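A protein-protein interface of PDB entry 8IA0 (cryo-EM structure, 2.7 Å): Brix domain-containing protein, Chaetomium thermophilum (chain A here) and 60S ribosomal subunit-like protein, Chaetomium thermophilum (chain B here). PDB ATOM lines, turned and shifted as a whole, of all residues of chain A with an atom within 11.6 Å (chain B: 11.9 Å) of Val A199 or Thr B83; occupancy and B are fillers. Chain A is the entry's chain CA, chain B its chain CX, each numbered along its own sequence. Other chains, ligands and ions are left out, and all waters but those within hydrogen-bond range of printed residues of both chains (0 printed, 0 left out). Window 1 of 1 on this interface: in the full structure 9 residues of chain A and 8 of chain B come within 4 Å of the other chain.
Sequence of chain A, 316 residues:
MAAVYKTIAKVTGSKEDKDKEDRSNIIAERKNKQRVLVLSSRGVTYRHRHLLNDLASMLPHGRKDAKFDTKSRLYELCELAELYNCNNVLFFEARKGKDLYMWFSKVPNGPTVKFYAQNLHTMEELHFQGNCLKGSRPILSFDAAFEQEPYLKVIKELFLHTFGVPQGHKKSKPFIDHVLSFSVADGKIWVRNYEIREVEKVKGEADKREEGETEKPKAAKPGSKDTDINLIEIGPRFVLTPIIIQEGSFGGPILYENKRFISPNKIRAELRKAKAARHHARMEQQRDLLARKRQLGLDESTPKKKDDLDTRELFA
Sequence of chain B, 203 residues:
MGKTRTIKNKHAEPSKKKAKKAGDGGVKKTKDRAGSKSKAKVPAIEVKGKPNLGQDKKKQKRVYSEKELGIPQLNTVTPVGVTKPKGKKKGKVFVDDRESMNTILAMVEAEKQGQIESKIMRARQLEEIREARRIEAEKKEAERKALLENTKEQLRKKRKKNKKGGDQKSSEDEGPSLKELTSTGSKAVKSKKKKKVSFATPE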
ATOM      1  N   GLN A 129       3.638 -21.815  18.988  1.00  0.00           N
ATOM      2  CA  GLN A 129       3.687 -20.444  19.493  1.00  0.00           C
ATOM      3  C   GLN A 129       2.606 -20.135  20.518  1.00  0.00           C
ATOM      4  O   GLN A 129       2.383 -18.960  20.832  1.00  0.00           O
ATOM      5  CB  GLN A 129       3.599 -19.414  18.360  1.00  0.00           C
ATOM      6  CG  GLN A 129       4.690 -19.533  17.319  1.00  0.00           C
ATOM      7  CD  GLN A 129       4.317 -18.861  16.018  1.00  0.00           C
ATOM      8  OE1 GLN A 129       3.775 -17.756  16.010  1.00  0.00           O
ATOM      9  NE2 GLN A 129       4.603 -19.526  14.906  1.00  0.00           N
ATOM     10  N   ASN A 131       0.496 -21.299  24.367  1.00  0.00           N
ATOM     11  CA  ASN A 131       0.615 -21.966  25.653  1.00  0.00           C
ATOM     12  C   ASN A 131      -0.628 -21.673  26.475  1.00  0.00           C
ATOM     13  O   ASN A 131      -1.366 -20.723  26.203  1.00  0.00           O
ATOM     14  CB  ASN A 131       1.875 -21.522  26.401  1.00  0.00           C
ATOM     15  CG  ASN A 131       2.537 -22.655  27.151  1.00  0.00           C
ATOM     16  OD1 ASN A 131       1.987 -23.748  27.254  1.00  0.00           O
ATOM     17  ND2 ASN A 131       3.726 -22.401  27.678  1.00  0.00           N
ATOM     18  N   ASP A 177      -8.101 -19.824  29.571  1.00  0.00           N
ATOM     19  CA  ASP A 177      -7.277 -19.215  28.535  1.00  0.00           C
ATOM     20  C   ASP A 177      -7.095 -20.076  27.289  1.00  0.00           C
ATOM     21  O   ASP A 177      -6.329 -19.684  26.400  1.00  0.00           O
ATOM     22  CB  ASP A 177      -5.901 -18.862  29.105  1.00  0.00           C
ATOM     23  CG  ASP A 177      -5.257 -20.026  29.826  1.00  0.00           C
ATOM     24  OD1 ASP A 177      -5.983 -20.774  30.512  1.00  0.00           O
ATOM     25  OD2 ASP A 177      -4.027 -20.192  29.711  1.00  0.00           O
ATOM     26  N   GLU A 195      -5.034 -21.272  22.017  1.00  0.00           N
ATOM     27  CA  GLU A 195      -4.926 -20.348  23.138  1.00  0.00           C
ATOM     28  C   GLU A 195      -5.777 -19.116  22.880  1.00  0.00           C
ATOM     29  O   GLU A 195      -5.725 -18.526  21.798  1.00  0.00           O
ATOM     30  CB  GLU A 195      -3.475 -19.930  23.373  1.00  0.00           C
ATOM     31  CG  GLU A 195      -3.293 -18.699  24.231  1.00  0.00           C
ATOM     32  CD  GLU A 195      -1.959 -18.024  23.995  1.00  0.00           C
ATOM     33  OE1 GLU A 195      -1.650 -17.046  24.706  1.00  0.00           O
ATOM     34  OE2 GLU A 195      -1.217 -18.474  23.097  1.00  0.00           O
ATOM     35  N   ILE A 196      -6.558 -18.730  23.881  1.00  0.00           N
ATOM     36  CA  ILE A 196      -7.382 -17.532  23.804  1.00  0.00           C
ATOM     37  C   ILE A 196      -6.500 -16.341  24.156  1.00  0.00           C
ATOM     38  O   ILE A 196      -6.218 -16.090  25.331  1.00  0.00           O
ATOM     39  CB  ILE A 196      -8.597 -17.626  24.733  1.00  0.00           C
ATOM     40  CG1 ILE A 196      -9.412 -18.877  24.410  1.00  0.00           C
ATOM     41  CG2 ILE A 196      -9.456 -16.382  24.608  1.00  0.00           C
ATOM     42  CD1 ILE A 196     -10.700 -18.986  25.194  1.00  0.00           C
ATOM     43  N   ARG A 197      -6.064 -15.608  23.138  1.00  0.00           N
ATOM     44  CA  ARG A 197      -5.245 -14.419  23.320  1.00  0.00           C
ATOM     45  C   ARG A 197      -6.113 -13.180  23.158  1.00  0.00           C
ATOM     46  O   ARG A 197      -6.788 -13.019  22.136  1.00  0.00           O
ATOM     47  CB  ARG A 197      -4.089 -14.389  22.320  1.00  0.00           C
ATOM     48  CG  ARG A 197      -3.334 -13.075  22.300  1.00  0.00           C
ATOM     49  CD  ARG A 197      -2.203 -13.067  23.307  1.00  0.00           C
ATOM     50  NE  ARG A 197      -1.352 -14.242  23.183  1.00  0.00           N
ATOM     51  CZ  ARG A 197      -0.148 -14.237  22.629  1.00  0.00           C
ATOM     52  NH1 ARG A 197       0.373 -13.133  22.122  1.00  0.00           N
ATOM     53  NH2 ARG A 197       0.551 -15.366  22.582  1.00  0.00           N
ATOM     54  N   GLU A 198      -6.092 -12.312  24.163  1.00  0.00           N
ATOM     55  CA  GLU A 198      -6.896 -11.099  24.153  1.00  0.00           C
ATOM     56  C   GLU A 198      -6.050  -9.916  23.702  1.00  0.00           C
ATOM     57  O   GLU A 198      -4.918  -9.741  24.164  1.00  0.00           O
ATOM     58  CB  GLU A 198      -7.486 -10.836  25.535  1.00  0.00           C
ATOM     59  CG  GLU A 198      -8.567 -11.818  25.934  1.00  0.00           C
ATOM     60  CD  GLU A 198      -8.979 -11.671  27.383  1.00  0.00           C
ATOM     61  OE1 GLU A 198      -8.090 -11.702  28.257  1.00  0.00           O
ATOM     62  OE2 GLU A 198     -10.190 -11.522  27.648  1.00  0.00           O
ATOM     63  N   VAL A 199      -6.602  -9.113  22.798  1.00  0.00           N
ATOM     64  CA  VAL A 199      -5.934  -7.937  22.257  1.00  0.00           C
ATOM     65  C   VAL A 199      -6.836  -6.733  22.483  1.00  0.00           C
ATOM     66  O   VAL A 199      -8.061  -6.838  22.358  1.00  0.00           O
ATOM     67  CB  VAL A 199      -5.612  -8.102  20.761  1.00  0.00           C
ATOM     68  CG1 VAL A 199      -4.631  -7.032  20.309  1.00  0.00           C
ATOM     69  CG2 VAL A 199      -5.053  -9.484  20.488  1.00  0.00           C
ATOM     70  N   GLU A 200      -6.234  -5.598  22.831  1.00  0.00           N
ATOM     71  CA  GLU A 200      -7.004  -4.376  23.009  1.00  0.00           C
ATOM     72  C   GLU A 200      -7.588  -3.920  21.679  1.00  0.00           C
ATOM     73  O   GLU A 200      -6.902  -3.919  20.653  1.00  0.00           O
ATOM     74  CB  GLU A 200      -6.124  -3.280  23.607  1.00  0.00           C
ATOM     75  CG  GLU A 200      -5.801  -3.479  25.076  1.00  0.00           C
ATOM     76  CD  GLU A 200      -5.147  -2.262  25.698  1.00  0.00           C
ATOM     77  OE1 GLU A 200      -4.833  -1.308  24.954  1.00  0.00           O
ATOM     78  OE2 GLU A 200      -4.946  -2.258  26.930  1.00  0.00           O
ATOM     79  N   LYS A 201      -8.858  -3.531  21.701  1.00  0.00           N
ATOM     80  CA  LYS A 201      -9.525  -3.096  20.485  1.00  0.00           C
ATOM     81  C   LYS A 201      -9.045  -1.707  20.073  1.00  0.00           C
ATOM     82  O   LYS A 201      -8.589  -0.905  20.892  1.00  0.00           O
ATOM     83  CB  LYS A 201     -11.041  -3.093  20.674  1.00  0.00           C
ATOM     84  CG  LYS A 201     -11.773  -4.086  19.789  1.00  0.00           C
ATOM     85  CD  LYS A 201     -13.231  -4.220  20.192  1.00  0.00           C
ATOM     86  CE  LYS A 201     -13.375  -4.939  21.520  1.00  0.00           C
ATOM     87  NZ  LYS A 201     -14.783  -4.929  22.003  1.00  0.00           N
ATOM     88  N   VAL A 202      -9.154  -1.430  18.780  1.00  0.00           N
ATOM     89  CA  VAL A 202      -8.718  -0.162  18.212  1.00  0.00           C
ATOM     90  C   VAL A 202      -9.887   0.812  18.222  1.00  0.00           C
ATOM     91  O   VAL A 202     -10.985   0.486  17.755  1.00  0.00           O
ATOM     92  CB  VAL A 202      -8.172  -0.355  16.788  1.00  0.00           C
ATOM     93  CG1 VAL A 202      -7.796   0.984  16.177  1.00  0.00           C
ATOM     94  CG2 VAL A 202      -6.978  -1.292  16.804  1.00  0.00           C
ATOM     95  N   LYS A 203      -9.655   2.007  18.757  1.00  0.00           N
ATOM     96  CA  LYS A 203     -10.684   3.036  18.822  1.00  0.00           C
ATOM     97  C   LYS A 203     -11.072   3.518  17.429  1.00  0.00           C
ATOM     98  O   LYS A 203     -10.296   3.396  16.481  1.00  0.00           O
ATOM     99  CB  LYS A 203     -10.206   4.215  19.672  1.00  0.00           C
ATOM    100  CG  LYS A 203     -11.115   5.432  19.617  1.00  0.00           C
ATOM    101  CD  LYS A 203     -10.576   6.562  20.481  1.00  0.00           C
ATOM    102  CE  LYS A 203     -11.415   7.820  20.331  1.00  0.00           C
ATOM    103  NZ  LYS A 203     -11.268   8.427  18.979  1.00  0.00           N
ATOM    104  N   THR A 227     -12.134  -5.950  24.514  1.00  0.00           N
ATOM    105  CA  THR A 227     -10.991  -6.579  23.865  1.00  0.00           C
ATOM    106  C   THR A 227     -11.431  -7.737  22.976  1.00  0.00           C
ATOM    107  O   THR A 227     -12.279  -8.536  23.368  1.00  0.00           O
ATOM    108  CB  THR A 227      -9.974  -7.097  24.897  1.00  0.00           C
ATOM    109  OG1 THR A 227     -10.568  -8.142  25.676  1.00  0.00           O
ATOM    110  CG2 THR A 227      -9.531  -5.975  25.819  1.00  0.00           C
ATOM    111  N   ASP A 228     -10.860  -7.827  21.780  1.00  0.00           N
ATOM    112  CA  ASP A 228     -11.161  -8.916  20.864  1.00  0.00           C
ATOM    113  C   ASP A 228     -10.238 -10.102  21.130  1.00  0.00           C
ATOM    114  O   ASP A 228      -9.216  -9.992  21.811  1.00  0.00           O
ATOM    115  CB  ASP A 228     -11.055  -8.451  19.406  1.00  0.00           C
ATOM    116  CG  ASP A 228      -9.679  -7.917  19.052  1.00  0.00           C
ATOM    117  OD1 ASP A 228      -8.803  -7.856  19.936  1.00  0.00           O
ATOM    118  OD2 ASP A 228      -9.474  -7.555  17.875  1.00  0.00           O
ATOM    119  N   ILE A 229     -10.617 -11.253  20.582  1.00  0.00           N
ATOM    120  CA  ILE A 229      -9.950 -12.519  20.857  1.00  0.00           C
ATOM    121  C   ILE A 229      -9.244 -12.990  19.595  1.00  0.00           C
ATOM    122  O   ILE A 229      -9.853 -13.046  18.521  1.00  0.00           O
ATOM    123  CB  ILE A 229     -10.945 -13.586  21.348  1.00  0.00           C
ATOM    124  CG1 ILE A 229     -11.414 -13.269  22.765  1.00  0.00           C
ATOM    125  CG2 ILE A 229     -10.319 -14.968  21.292  1.00  0.00           C
ATOM    126  CD1 ILE A 229     -12.445 -14.236  23.291  1.00  0.00           C
ATOM    127  N   ASN A 230      -7.964 -13.320  19.727  1.00  0.00           N
ATOM    128  CA  ASN A 230      -7.209 -14.013  18.698  1.00  0.00           C
ATOM    129  C   ASN A 230      -6.787 -15.383  19.212  1.00  0.00           C
ATOM    130  O   ASN A 230      -6.474 -15.558  20.392  1.00  0.00           O
ATOM    131  CB  ASN A 230      -5.981 -13.205  18.268  1.00  0.00           C
ATOM    132  CG  ASN A 230      -6.330 -12.075  17.327  1.00  0.00           C
ATOM    133  OD1 ASN A 230      -5.898 -10.938  17.519  1.00  0.00           O
ATOM    134  ND2 ASN A 230      -7.120 -12.377  16.305  1.00  0.00           N
ATOM    135  N   LEU A 231      -6.783 -16.361  18.311  1.00  0.00           N
ATOM    136  CA  LEU A 231      -6.492 -17.744  18.659  1.00  0.00           C
ATOM    137  C   LEU A 231      -5.141 -18.159  18.096  1.00  0.00           C
ATOM    138  O   LEU A 231      -4.808 -17.841  16.952  1.00  0.00           O
ATOM    139  CB  LEU A 231      -7.576 -18.689  18.140  1.00  0.00           C
ATOM    140  CG  LEU A 231      -8.927 -18.646  18.849  1.00  0.00           C
ATOM    141  CD1 LEU A 231      -9.739 -19.877  18.499  1.00  0.00           C
ATOM    142  CD2 LEU A 231      -8.744 -18.532  20.351  1.00  0.00           C
ATOM    143  N   ILE A 232      -4.367 -18.868  18.913  1.00  0.00           N
ATOM    144  CA  ILE A 232      -3.082 -19.432  18.517  1.00  0.00           C
ATOM    145  C   ILE A 232      -3.091 -20.906  18.894  1.00  0.00           C
ATOM    146  O   ILE A 232      -3.446 -21.254  20.026  1.00  0.00           O
ATOM    147  CB  ILE A 232      -1.902 -18.708  19.187  1.00  0.00           C
ATOM    148  CG1 ILE A 232      -1.983 -17.202  18.938  1.00  0.00           C
ATOM    149  CG2 ILE A 232      -0.583 -19.257  18.681  1.00  0.00           C
ATOM    150  CD1 ILE A 232      -1.547 -16.369  20.117  1.00  0.00           C
ATOM    151  N   ILE B  71       8.486 -10.018  16.275  1.00  0.00           N
ATOM    152  CA  ILE B  71       8.490 -11.350  16.869  1.00  0.00           C
ATOM    153  C   ILE B  71       7.248 -11.481  17.747  1.00  0.00           C
ATOM    154  O   ILE B  71       7.034 -10.629  18.622  1.00  0.00           O
ATOM    155  CB  ILE B  71       9.768 -11.590  17.676  1.00  0.00           C
ATOM    156  CG1 ILE B  71      10.850 -12.164  16.768  1.00  0.00           C
ATOM    157  CG2 ILE B  71       9.512 -12.553  18.821  1.00  0.00           C
ATOM    158  CD1 ILE B  71      12.200 -12.211  17.409  1.00  0.00           C
ATOM    159  N   PRO B  72       6.410 -12.496  17.539  1.00  0.00           N
ATOM    160  CA  PRO B  72       5.215 -12.649  18.375  1.00  0.00           C
ATOM    161  C   PRO B  72       5.574 -12.881  19.834  1.00  0.00           C
ATOM    162  O   PRO B  72       6.577 -13.518  20.160  1.00  0.00           O
ATOM    163  CB  PRO B  72       4.513 -13.873  17.774  1.00  0.00           C
ATOM    164  CG  PRO B  72       5.075 -14.008  16.399  1.00  0.00           C
ATOM    165  CD  PRO B  72       6.482 -13.518  16.483  1.00  0.00           C
ATOM    166  N   GLN B  73       4.733 -12.352  20.718  1.00  0.00           N
ATOM    167  CA  GLN B  73       4.911 -12.545  22.149  1.00  0.00           C
ATOM    168  C   GLN B  73       4.362 -13.900  22.578  1.00  0.00           C
ATOM    169  O   GLN B  73       3.310 -14.338  22.107  1.00  0.00           O
ATOM    170  CB  GLN B  73       4.235 -11.416  22.923  1.00  0.00           C
ATOM    171  CG  GLN B  73       4.234 -10.100  22.172  1.00  0.00           C
ATOM    172  CD  GLN B  73       3.496  -9.006  22.907  1.00  0.00           C
ATOM    173  OE1 GLN B  73       4.021  -8.407  23.843  1.00  0.00           O
ATOM    174  NE2 GLN B  73       2.283  -8.713  22.461  1.00  0.00           N
ATOM    175  N   LEU B  74       5.085 -14.558  23.477  1.00  0.00           N
ATOM    176  CA  LEU B  74       4.831 -15.946  23.834  1.00  0.00           C
ATOM    177  C   LEU B  74       4.297 -16.044  25.256  1.00  0.00           C
ATOM    178  O   LEU B  74       4.781 -15.358  26.161  1.00  0.00           O
ATOM    179  CB  LEU B  74       6.108 -16.778  23.702  1.00  0.00           C
ATOM    180  CG  LEU B  74       6.264 -17.612  22.430  1.00  0.00           C
ATOM    181  CD1 LEU B  74       5.846 -16.825  21.199  1.00  0.00           C
ATOM    182  CD2 LEU B  74       7.690 -18.111  22.289  1.00  0.00           C
ATOM    183  N   ASN B  75       3.310 -16.914  25.450  1.00  0.00           N
ATOM    184  CA  ASN B  75       2.735 -17.134  26.769  1.00  0.00           C
ATOM    185  C   ASN B  75       3.614 -18.092  27.558  1.00  0.00           C
ATOM    186  O   ASN B  75       3.953 -19.178  27.081  1.00  0.00           O
ATOM    187  CB  ASN B  75       1.318 -17.688  26.648  1.00  0.00           C
ATOM    188  CG  ASN B  75       0.496 -17.458  27.897  1.00  0.00           C
ATOM    189  OD1 ASN B  75       0.771 -16.551  28.678  1.00  0.00           O
ATOM    190  ND2 ASN B  75      -0.529 -18.280  28.089  1.00  0.00           N
ATOM    191  N   THR B  76       3.985 -17.688  28.768  1.00  0.00           N
ATOM    192  CA  THR B  76       4.933 -18.432  29.585  1.00  0.00           C
ATOM    193  C   THR B  76       4.418 -18.373  31.022  1.00  0.00           C
ATOM    194  O   THR B  76       3.277 -17.968  31.270  1.00  0.00           O
ATOM    195  CB  THR B  76       6.340 -17.842  29.387  1.00  0.00           C
ATOM    196  OG1 THR B  76       6.590 -17.690  27.985  1.00  0.00           O
ATOM    197  CG2 THR B  76       7.417 -18.765  29.925  1.00  0.00           C
ATOM    198  N   THR B  78       5.374 -16.272  33.027  1.00  0.00           N
ATOM    199  CA  THR B  78       5.045 -14.855  33.058  1.00  0.00           C
ATOM    200  C   THR B  78       3.908 -14.588  32.081  1.00  0.00           C
ATOM    201  O   THR B  78       4.087 -14.783  30.874  1.00  0.00           O
ATOM    202  CB  THR B  78       6.256 -14.012  32.691  1.00  0.00           C
ATOM    203  OG1 THR B  78       7.444 -14.641  33.186  1.00  0.00           O
ATOM    204  CG2 THR B  78       6.136 -12.622  33.296  1.00  0.00           C
ATOM    205  N   PRO B  79       2.740 -14.155  32.547  1.00  0.00           N
ATOM    206  CA  PRO B  79       1.598 -13.996  31.642  1.00  0.00           C
ATOM    207  C   PRO B  79       1.836 -12.922  30.594  1.00  0.00           C
ATOM    208  O   PRO B  79       2.460 -11.890  30.852  1.00  0.00           O
ATOM    209  CB  PRO B  79       0.452 -13.603  32.582  1.00  0.00           C
ATOM    210  CG  PRO B  79       0.908 -14.008  33.946  1.00  0.00           C
ATOM    211  CD  PRO B  79       2.389 -13.853  33.941  1.00  0.00           C
ATOM    212  N   VAL B  80       1.321 -13.180  29.389  1.00  0.00           N
ATOM    213  CA  VAL B  80       1.348 -12.164  28.344  1.00  0.00           C
ATOM    214  C   VAL B  80       0.387 -11.034  28.672  1.00  0.00           C
ATOM    215  O   VAL B  80       0.656  -9.869  28.355  1.00  0.00           O
ATOM    216  CB  VAL B  80       1.027 -12.785  26.972  1.00  0.00           C
ATOM    217  CG1 VAL B  80       2.267 -13.421  26.377  1.00  0.00           C
ATOM    218  CG2 VAL B  80      -0.089 -13.803  27.098  1.00  0.00           C
ATOM    219  N   GLY B  81      -0.738 -11.347  29.304  1.00  0.00           N
ATOM    220  CA  GLY B  81      -1.733 -10.336  29.579  1.00  0.00           C
ATOM    221  C   GLY B  81      -2.456  -9.915  28.311  1.00  0.00           C
ATOM    222  O   GLY B  81      -2.443 -10.600  27.286  1.00  0.00           O
ATOM    223  N   VAL B  82      -3.099  -8.753  28.394  1.00  0.00           N
ATOM    224  CA  VAL B  82      -3.798  -8.183  27.249  1.00  0.00           C
ATOM    225  C   VAL B  82      -2.765  -7.474  26.382  1.00  0.00           C
ATOM    226  O   VAL B  82      -2.153  -6.492  26.805  1.00  0.00           O
ATOM    227  CB  VAL B  82      -4.911  -7.226  27.685  1.00  0.00           C
ATOM    228  CG1 VAL B  82      -5.938  -7.074  26.577  1.00  0.00           C
ATOM    229  CG2 VAL B  82      -5.569  -7.729  28.957  1.00  0.00           C
ATOM    230  N   THR B  83      -2.569  -7.975  25.168  1.00  0.00           N
ATOM    231  CA  THR B  83      -1.572  -7.425  24.269  1.00  0.00           C
ATOM    232  C   THR B  83      -2.168  -6.287  23.445  1.00  0.00           C
ATOM    233  O   THR B  83      -3.382  -6.195  23.249  1.00  0.00           O
ATOM    234  CB  THR B  83      -1.026  -8.514  23.350  1.00  0.00           C
ATOM    235  OG1 THR B  83      -2.115  -9.167  22.689  1.00  0.00           O
ATOM    236  CG2 THR B  83      -0.272  -9.549  24.167  1.00  0.00           C
ATOM    237  N   LYS B  84      -1.293  -5.408  22.964  1.00  0.00           N
ATOM    238  CA  LYS B  84      -1.748  -4.255  22.207  1.00  0.00           C
ATOM    239  C   LYS B  84      -1.385  -4.402  20.736  1.00  0.00           C
ATOM    240  O   LYS B  84      -0.298  -4.897  20.415  1.00  0.00           O
ATOM    241  CB  LYS B  84      -1.133  -2.961  22.752  1.00  0.00           C
ATOM    242  CG  LYS B  84      -1.592  -2.599  24.151  1.00  0.00           C
ATOM    243  CD  LYS B  84      -0.570  -1.719  24.848  1.00  0.00           C
ATOM    244  CE  LYS B  84      -0.886  -1.555  26.324  1.00  0.00           C
ATOM    245  NZ  LYS B  84      -2.167  -2.210  26.699  1.00  0.00           N
ATOM    246  N   PRO B  85      -2.265  -3.992  19.826  1.00  0.00           N
ATOM    247  CA  PRO B  85      -1.952  -4.098  18.397  1.00  0.00           C
ATOM    248  C   PRO B  85      -0.774  -3.219  18.010  1.00  0.00           C
ATOM    249  O   PRO B  85      -0.566  -2.136  18.562  1.00  0.00           O
ATOM    250  CB  PRO B  85      -3.242  -3.631  17.715  1.00  0.00           C
ATOM    251  CG  PRO B  85      -3.944  -2.813  18.745  1.00  0.00           C
ATOM    252  CD  PRO B  85      -3.606  -3.434  20.061  1.00  0.00           C
ATOM    253  N   LYS B  86       0.000  -3.702  17.043  1.00  0.00           N
ATOM    254  CA  LYS B  86       1.189  -2.993  16.595  1.00  0.00           C
ATOM    255  C   LYS B  86       0.809  -1.816  15.707  1.00  0.00           C
ATOM    256  O   LYS B  86      -0.148  -1.885  14.933  1.00  0.00           O
ATOM    257  CB  LYS B  86       2.123  -3.939  15.841  1.00  0.00           C
ATOM    258  CG  LYS B  86       3.467  -3.331  15.474  1.00  0.00           C
ATOM    259  CD  LYS B  86       4.418  -3.341  16.659  1.00  0.00           C
ATOM    260  CE  LYS B  86       5.289  -4.586  16.659  1.00  0.00           C
ATOM    261  NZ  LYS B  86       6.311  -4.548  15.577  1.00  0.00           N
ATOM    262  N   GLY B  87       1.569  -0.729  15.825  1.00  0.00           N
ATOM    263  CA  GLY B  87       1.308   0.453  15.033  1.00  0.00           C
ATOM    264  C   GLY B  87       0.083   1.229  15.443  1.00  0.00           C
ATOM    265  O   GLY B  87      -0.455   1.990  14.634  1.00  0.00           O
ATOM    266  N   LYS B  88      -0.380   1.063  16.677  1.00  0.00           N
ATOM    267  CA  LYS B  88      -1.582   1.721  17.161  1.00  0.00           C
ATOM    268  C   LYS B  88      -1.278   2.419  18.481  1.00  0.00           C
ATOM    269  O   LYS B  88      -0.176   2.321  19.027  1.00  0.00           O
ATOM    270  CB  LYS B  88      -2.734   0.722  17.317  1.00  0.00           C
ATOM    271  CG  LYS B  88      -3.283   0.207  15.998  1.00  0.00           C
ATOM    272  CD  LYS B  88      -4.068   1.283  15.270  1.00  0.00           C
ATOM    273  CE  LYS B  88      -4.460   0.834  13.874  1.00  0.00           C
ATOM    274  NZ  LYS B  88      -4.261  -0.628  13.683  1.00  0.00           N
ATOM    275  N   LYS B  89      -2.276   3.133  18.989  1.00  0.00           N
ATOM    276  CA  LYS B  89      -2.137   3.937  20.200  1.00  0.00           C
ATOM    277  C   LYS B  89      -2.052   3.031  21.419  1.00  0.00           C
ATOM    278  O   LYS B  89      -3.065   2.526  21.904  1.00  0.00           O
ATOM    279  CB  LYS B  89      -3.311   4.898  20.325  1.00  0.00           C
ATOM    280  CG  LYS B  89      -3.115   5.975  21.367  1.00  0.00           C
ATOM    281  CD  LYS B  89      -4.298   6.920  21.415  1.00  0.00           C
ATOM    282  CE  LYS B  89      -5.097   6.726  22.685  1.00  0.00           C
ATOM    283  NZ  LYS B  89      -4.797   7.797  23.672  1.00  0.00           N
ATOM    284  N   LYS B  90      -0.842   2.822  21.927  1.00  0.00           N
ATOM    285  CA  LYS B  90      -0.672   2.198  23.234  1.00  0.00           C
ATOM    286  C   LYS B  90      -0.805   3.288  24.291  1.00  0.00           C
ATOM    287  O   LYS B  90       0.100   4.109  24.472  1.00  0.00           O
ATOM    288  CB  LYS B  90       0.662   1.459  23.316  1.00  0.00           C
ATOM    289  CG  LYS B  90       1.887   2.274  22.951  1.00  0.00           C
ATOM    290  CD  LYS B  90       3.168   1.556  23.334  1.00  0.00           C
ATOM    291  CE  LYS B  90       3.370   0.308  22.498  1.00  0.00           C
ATOM    292  NZ  LYS B  90       3.526   0.632  21.054  1.00  0.00           N
ATOM    293  N   GLY B  91      -1.946   3.311  24.974  1.00  0.00           N
ATOM    294  CA  GLY B  91      -2.279   4.397  25.874  1.00  0.00           C
ATOM    295  C   GLY B  91      -1.264   4.638  26.970  1.00  0.00           C
ATOM    296  O   GLY B  91      -0.846   3.702  27.658  1.00  0.00           O
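The backbone NH (N) of Thr B83 lies within hydrogen-bond range of the backbone carbonyl oxygen (O) of Glu A198 (3.1 Å). O of Gln B73 is in hydrogen-bond range of NH2 of Arg A197, 3.0 Å away. O of Thr B83 lies within hydrogen-bond range of N of Glu A200 (2.9 Å). The side-chain carboxylate (OE2) of Glu A200 is in salt-bridge range of the side-chain amino group (NZ) of Lys B84, 2.8 Å away. O of Asn A131 lies within hydrogen-bond range of ND2 of Asn B75 (3.2 Å).
OE1 of Glu A195 lies within salt-bridge range of NE of Arg A197 (3.2 Å). The side-chain amide oxygen of Asn B75 lies close to the backbone NH of Val B80, 3.5 Å away. The backbone NH of Glu A195 lies within hydrogen-bond range of the backbone carbonyl oxygen of Ile A232, 2.5 Å away. N of Val A199 lies within hydrogen-bond range of O of Asp A228 (2.9 Å). The backbone NH (N) of Asn A230 is in hydrogen-bond range of the backbone carbonyl oxygen (O) of Arg A197, 2.7 Å away.
Pro B72 touches Gln A129 (CG to OE1, 3.99 Å). Glu A195 touches Asn B75. Arg A197 touches Thr B83 (CD to OG1, 3.9 Å). Glu A198 touches Val B82 (O to CA, 3.6 Å). O of Thr B83 touches CA of Val A199 (3.2 Å). CG1 of Val B82 touches CG of Glu A200, at 3.9 Å. CD of Pro B85 touches O of Glu A200 (3.4 Å). Val A202 touches Pro B85. CG1 of Val A202 touches CD of Lys B88, 3.8 Å away. CG2 of Thr A227 touches CG1 of Val B82, 3.8 Å away.
Thr B83 touches four residues of chain A. Arg A197 touches just these residues of chain B: Gln B73 and Thr B83. Of chain B, only Val B82 (3.6 Å) and Thr B83 (3.1 Å) come within 4 Å of Glu A198. No residue of chain B comes within 4 Å of Lys A201. Of chain B, only Val B82 comes within 4 Å of Thr A227. No residue of chain B comes within 4 Å of Asn A230. Gln B73 touches just one residue of chain A: Arg A197. No residue of chain A comes within 4 Å of Val B80. Gly B81 touches none of the printed residues of chain A. Val B82 touches just these residues of chain A: Glu A198, Glu A200 and Thr A227. Lys B84 touches one residue of chain A. Of the printed residues of chain A, Pro B72 touches Gln A129. Printed residues of chain A within 4 Å of Asn B75: Asn A131 (3.2 Å) and Glu A195 (3.6 Å). Of the printed residues of chain B, Asn A131 touches Asn B75 (3.2 Å). Printed residues of chain B within 4 Å of Gln A129: Pro B72 (3.99 Å). Gly B87 touches none of the printed residues of chain A. The nearest residue of chain A that does not touch Thr B83 is Lys A201 (6.3 Å).
Hydrophobic or aromatic side chains of chain A within 4 Å of the printed part of chain B: Val A199 and Val A202. Of the 20 printed residues of chain B, 8 touch a printed residue of chain A. Hydrophobic or aromatic side chains of chain B that line the printed part of chain A: Pro B72, Val B82 and Pro B85. Among the printed residues, Asp or Glu carboxylates within 4 Å of a Lys or Arg side-chain nitrogen of the other chain: Glu A200 with Lys B84.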
